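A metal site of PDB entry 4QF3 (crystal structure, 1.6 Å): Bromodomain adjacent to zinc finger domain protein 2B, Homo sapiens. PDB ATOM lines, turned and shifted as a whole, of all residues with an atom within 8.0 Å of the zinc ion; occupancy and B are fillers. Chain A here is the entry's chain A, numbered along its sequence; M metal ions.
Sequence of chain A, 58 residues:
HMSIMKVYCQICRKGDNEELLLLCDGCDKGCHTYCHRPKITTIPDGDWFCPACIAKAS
The zinc ion is bound by a ring nitrogen (ND1) of His 32, 2.1 Å away. SG of Cys 12 is bound to the zinc ion, at 2.3 Å. The side-chain sulfur (SG) of Cys 35 binds the zinc ion (2.3 Å). SG of Cys 9 is bound to the zinc ion (2.3 Å).
Four residues have an atom within 4 Å of the zinc ion: Cys 9, Cys 12, His 32 and Cys 35. The nearest printed residue that does not touch the zinc ion is Tyr 34 (4.3 Å).
A ring nitrogen (NE2) of His 32 sits close to the side-chain hydroxyl (OH) of Tyr 34, 3.3 Å away. NE2 of His 32 is in hydrogen-bond range of O of Asp 16, at 2.8 Å. SG of Cys 12 sits close to N of Lys 14. The side-chain sulfur of Cys 9 sits close to the backbone NH of Ile 11 (3.4 Å). O of Lys 14 sits at hydrogen-bond distance from N of Cys 9 (2.9 Å).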
ATOM      1  N   TYR A   8       1.007  14.691   1.209  1.00  0.00           N
ATOM      2  CA  TYR A   8       1.297  15.117   2.576  1.00  0.00           C
ATOM      3  C   TYR A   8       2.178  14.021   3.203  1.00  0.00           C
ATOM      4  O   TYR A   8       2.093  12.854   2.823  1.00  0.00           O
ATOM      5  CB  TYR A   8       0.007  15.418   3.382  1.00  0.00           C
ATOM      6  CG  TYR A   8      -0.883  16.607   2.908  1.00  0.00           C
ATOM      7  CD1 TYR A   8      -0.825  17.853   3.523  1.00  0.00           C
ATOM      8  CD2 TYR A   8      -1.803  16.456   1.881  1.00  0.00           C
ATOM      9  CE1 TYR A   8      -1.599  18.908   3.090  1.00  0.00           C
ATOM     10  CE2 TYR A   8      -2.605  17.489   1.469  1.00  0.00           C
ATOM     11  CZ  TYR A   8      -2.478  18.722   2.067  1.00  0.00           C
ATOM     12  OH  TYR A   8      -3.315  19.722   1.604  1.00  0.00           O
ATOM     13  N   CYS A   9       2.992  14.403   4.150  1.00  0.00           N
ATOM     14  CA  CYS A   9       3.825  13.414   4.880  1.00  0.00           C
ATOM     15  C   CYS A   9       2.955  12.463   5.728  1.00  0.00           C
ATOM     16  O   CYS A   9       2.038  12.907   6.442  1.00  0.00           O
ATOM     17  CB  CYS A   9       4.719  14.178   5.817  1.00  0.00           C
ATOM     18  SG  CYS A   9       5.726  13.147   6.923  1.00  0.00           S
ATOM     19  N   GLN A  10       3.184  11.143   5.630  1.00  0.00           N
ATOM     20  CA  GLN A  10       2.396  10.165   6.407  1.00  0.00           C
ATOM     21  C   GLN A  10       2.487  10.378   7.897  1.00  0.00           C
ATOM     22  O   GLN A  10       1.536  10.057   8.630  1.00  0.00           O
ATOM     23  CB  GLN A  10       2.904   8.760   6.105  1.00  0.00           C
ATOM     24  CG  GLN A  10       2.663   8.326   4.700  1.00  0.00           C
ATOM     25  CD  GLN A  10       1.211   7.919   4.510  1.00  0.00           C
ATOM     26  OE1 GLN A  10       0.404   8.663   3.921  1.00  0.00           O
ATOM     27  NE2 GLN A  10       0.852   6.752   5.050  1.00  0.00           N
ATOM     28  N   ILE A  11       3.573  10.983   8.375  1.00  0.00           N
ATOM     29  CA  ILE A  11       3.774  11.159   9.833  1.00  0.00           C
ATOM     30  C   ILE A  11       3.257  12.517  10.349  1.00  0.00           C
ATOM     31  O   ILE A  11       2.424  12.560  11.267  1.00  0.00           O
ATOM     32  CB  ILE A  11       5.279  10.969  10.190  1.00  0.00           C
ATOM     33  CG1 ILE A  11       5.752   9.555   9.792  1.00  0.00           C
ATOM     34  CG2 ILE A  11       5.500  11.286  11.668  1.00  0.00           C
ATOM     35  CD1 ILE A  11       5.086   8.427  10.534  1.00  0.00           C
ATOM     36  N   CYS A  12       3.710  13.628   9.779  1.00  0.00           N
ATOM     37  CA  CYS A  12       3.306  14.945  10.317  1.00  0.00           C
ATOM     38  C   CYS A  12       2.066  15.508   9.606  1.00  0.00           C
ATOM     39  O   CYS A  12       1.462  16.502  10.072  1.00  0.00           O
ATOM     40  CB  CYS A  12       4.455  15.942  10.222  1.00  0.00           C
ATOM     41  SG  CYS A  12       4.916  16.422   8.563  1.00  0.00           S
ATOM     42  N   ARG A  13       1.708  14.888   8.487  1.00  0.00           N
ATOM     43  CA  ARG A  13       0.534  15.262   7.640  1.00  0.00           C
ATOM     44  C   ARG A  13       0.621  16.644   7.022  1.00  0.00           C
ATOM     45  O   ARG A  13      -0.398  17.250   6.630  1.00  0.00           O
ATOM     46  CB  ARG A  13      -0.764  15.156   8.442  1.00  0.00           C
ATOM     47  CG  ARG A  13      -0.772  14.022   9.433  1.00  0.00           C
ATOM     48  CD  ARG A  13      -0.378  12.693   8.842  1.00  0.00           C
ATOM     49  NE  ARG A  13      -1.542  12.254   8.159  1.00  0.00           N
ATOM     50  CZ  ARG A  13      -1.831  11.023   7.778  1.00  0.00           C
ATOM     51  NH1 ARG A  13      -0.990  10.036   7.930  1.00  0.00           N
ATOM     52  NH2 ARG A  13      -3.007  10.816   7.208  1.00  0.00           N
ATOM     53  N   LYS A  14       1.819  17.170   6.946  1.00  0.00           N
ATOM     54  CA  LYS A  14       2.086  18.442   6.258  1.00  0.00           C
ATOM     55  C   LYS A  14       2.726  18.222   4.891  1.00  0.00           C
ATOM     56  O   LYS A  14       3.453  17.243   4.684  1.00  0.00           O
ATOM     57  CB  LYS A  14       2.929  19.346   7.123  1.00  0.00           C
ATOM     58  CG  LYS A  14       2.403  19.473   8.542  1.00  0.00           C
ATOM     59  CD  LYS A  14       3.247  20.414   9.404  1.00  0.00           C
ATOM     60  CE  LYS A  14       2.698  21.833   9.407  1.00  0.00           C
ATOM     61  NZ  LYS A  14       3.127  22.552  10.637  1.00  0.00           N
ATOM     62  N   GLY A  15       2.527  19.156   3.974  1.00  0.00           N
ATOM     63  CA  GLY A  15       3.104  19.075   2.614  1.00  0.00           C
ATOM     64  C   GLY A  15       4.167  20.114   2.314  1.00  0.00           C
ATOM     65  O   GLY A  15       4.508  20.383   1.142  1.00  0.00           O
ATOM     66  N   ASP A  16       4.744  20.678   3.358  1.00  0.00           N
ATOM     67  CA  ASP A  16       5.844  21.614   3.208  1.00  0.00           C
ATOM     68  C   ASP A  16       7.199  20.926   2.965  1.00  0.00           C
ATOM     69  O   ASP A  16       7.283  19.688   2.968  1.00  0.00           O
ATOM     70  CB  ASP A  16       5.913  22.550   4.451  1.00  0.00           C
ATOM     71  CG  ASP A  16       6.212  21.810   5.768  1.00  0.00           C
ATOM     72  OD1 ASP A  16       6.129  20.559   5.855  1.00  0.00           O
ATOM     73  OD2 ASP A  16       6.514  22.480   6.756  1.00  0.00           O
ATOM     74  N   ASN A  17       8.271  21.710   2.812  1.00  0.00           N
ATOM     75  CA  ASN A  17       9.616  21.166   2.693  1.00  0.00           C
ATOM     76  C   ASN A  17       9.652  20.111   1.613  1.00  0.00           C
ATOM     77  O   ASN A  17      10.112  18.980   1.834  1.00  0.00           O
ATOM     78  CB  ASN A  17      10.100  20.554   4.012  1.00  0.00           C
ATOM     79  CG  ASN A  17      10.848  21.523   4.889  1.00  0.00           C
ATOM     80  OD1 ASN A  17      10.601  21.603   6.102  1.00  0.00           O
ATOM     81  ND2 ASN A  17      11.781  22.262   4.301  1.00  0.00           N
ATOM     82  N   LEU A  20      12.531  17.714   0.851  1.00  0.00           N
ATOM     83  CA  LEU A  20      12.761  16.714   1.892  1.00  0.00           C
ATOM     84  C   LEU A  20      11.568  15.760   2.055  1.00  0.00           C
ATOM     85  O   LEU A  20      11.643  14.805   2.858  1.00  0.00           O
ATOM     86  CB  LEU A  20      13.053  17.406   3.231  1.00  0.00           C
ATOM     87  CG  LEU A  20      14.305  18.320   3.228  1.00  0.00           C
ATOM     88  CD1 LEU A  20      14.404  19.021   4.573  1.00  0.00           C
ATOM     89  CD2 LEU A  20      15.587  17.579   2.878  1.00  0.00           C
ATOM     90  N   LEU A  21      10.492  16.021   1.329  1.00  0.00           N
ATOM     91  CA  LEU A  21       9.328  15.170   1.389  1.00  0.00           C
ATOM     92  C   LEU A  21       9.496  14.082   0.326  1.00  0.00           C
ATOM     93  O   LEU A  21       9.226  14.257  -0.876  1.00  0.00           O
ATOM     94  CB  LEU A  21       8.073  16.035   1.216  1.00  0.00           C
ATOM     95  CG  LEU A  21       6.742  15.308   1.173  1.00  0.00           C
ATOM     96  CD1 LEU A  21       6.532  14.565   2.452  1.00  0.00           C
ATOM     97  CD2 LEU A  21       5.626  16.332   0.960  1.00  0.00           C
ATOM     98  N   GLY A  30       4.127   9.691   0.896  1.00  0.00           N
ATOM     99  CA  GLY A  30       5.186  10.653   1.225  1.00  0.00           C
ATOM    100  C   GLY A  30       5.611  10.610   2.668  1.00  0.00           C
ATOM    101  O   GLY A  30       4.853  10.260   3.568  1.00  0.00           O
ATOM    102  N   CYS A  31       6.893  10.925   2.910  1.00  0.00           N
ATOM    103  CA  CYS A  31       7.350  11.078   4.255  1.00  0.00           C
ATOM    104  C   CYS A  31       8.593  11.943   4.271  1.00  0.00           C
ATOM    105  O   CYS A  31       9.532  11.706   3.499  1.00  0.00           O
ATOM    106  CB  CYS A  31       7.642   9.723   4.889  1.00  0.00           C
ATOM    107  SG  CYS A  31       7.941   9.709   6.677  1.00  0.00           S
ATOM    108  N   HIS A  32       8.652  12.921   5.162  1.00  0.00           N
ATOM    109  CA  HIS A  32       9.872  13.746   5.259  1.00  0.00           C
ATOM    110  C   HIS A  32      11.071  12.981   5.804  1.00  0.00           C
ATOM    111  O   HIS A  32      10.918  12.127   6.661  1.00  0.00           O
ATOM    112  CB  HIS A  32       9.657  14.894   6.241  1.00  0.00           C
ATOM    113  CG  HIS A  32       8.675  15.931   5.763  1.00  0.00           C
ATOM    114  ND1 HIS A  32       7.445  16.140   6.361  1.00  0.00           N
ATOM    115  CD2 HIS A  32       8.745  16.799   4.732  1.00  0.00           C
ATOM    116  CE1 HIS A  32       6.832  17.136   5.749  1.00  0.00           C
ATOM    117  NE2 HIS A  32       7.597  17.555   4.750  1.00  0.00           N
ATOM    118  N   THR A  33      12.240  13.335   5.294  1.00  0.00           N
ATOM    119  CA  THR A  33      13.464  12.755   5.803  1.00  0.00           C
ATOM    120  C   THR A  33      13.491  12.795   7.347  1.00  0.00           C
ATOM    121  O   THR A  33      13.828  11.802   8.028  1.00  0.00           O
ATOM    122  CB  THR A  33      14.634  13.572   5.235  1.00  0.00           C
ATOM    123  OG1 THR A  33      14.405  14.961   5.473  1.00  0.00           O
ATOM    124  CG2 THR A  33      14.913  13.303   3.773  1.00  0.00           C
ATOM    125  N   TYR A  34      13.108  13.941   7.930  1.00  0.00           N
ATOM    126  CA  TYR A  34      13.231  14.187   9.358  1.00  0.00           C
ATOM    127  C   TYR A  34      12.071  13.665  10.186  1.00  0.00           C
ATOM    128  O   TYR A  34      12.095  13.749  11.402  1.00  0.00           O
ATOM    129  CB  TYR A  34      13.416  15.706   9.599  1.00  0.00           C
ATOM    130  CG  TYR A  34      12.345  16.569   8.936  1.00  0.00           C
ATOM    131  CD1 TYR A  34      11.061  16.670   9.475  1.00  0.00           C
ATOM    132  CD2 TYR A  34      12.605  17.252   7.783  1.00  0.00           C
ATOM    133  CE1 TYR A  34      10.096  17.452   8.883  1.00  0.00           C
ATOM    134  CE2 TYR A  34      11.659  18.072   7.200  1.00  0.00           C
ATOM    135  CZ  TYR A  34      10.391  18.149   7.749  1.00  0.00           C
ATOM    136  OH  TYR A  34       9.433  18.943   7.095  1.00  0.00           O
ATOM    137  N   CYS A  35      11.061  13.135   9.489  1.00  0.00           N
ATOM    138  CA  CYS A  35       9.898  12.478  10.120  1.00  0.00           C
ATOM    139  C   CYS A  35      10.060  10.974  10.183  1.00  0.00           C
ATOM    140  O   CYS A  35       9.428  10.335  11.019  1.00  0.00           O
ATOM    141  CB  CYS A  35       8.578  12.808   9.408  1.00  0.00           C
ATOM    142  SG  CYS A  35       8.090  14.537   9.657  1.00  0.00           S
ATOM    143  N   HIS A  36      10.954  10.380   9.354  1.00  0.00           N
ATOM    144  CA  HIS A  36      11.341   9.005   9.557  1.00  0.00           C
ATOM    145  C   HIS A  36      12.073   8.819  10.856  1.00  0.00           C
ATOM    146  O   HIS A  36      12.742   9.722  11.357  1.00  0.00           O
ATOM    147  CB  HIS A  36      12.318   8.549   8.485  1.00  0.00           C
ATOM    148  CG  HIS A  36      11.695   8.254   7.176  1.00  0.00           C
ATOM    149  ND1 HIS A  36      11.188   7.015   6.858  1.00  0.00           N
ATOM    150  CD2 HIS A  36      11.506   9.034   6.085  1.00  0.00           C
ATOM    151  CE1 HIS A  36      10.728   7.032   5.617  1.00  0.00           C
ATOM    152  NE2 HIS A  36      10.919   8.238   5.132  1.00  0.00           N
HETATM  153 ZN    ZN M   1       6.607  15.038   8.003  1.00  0.00          ZN
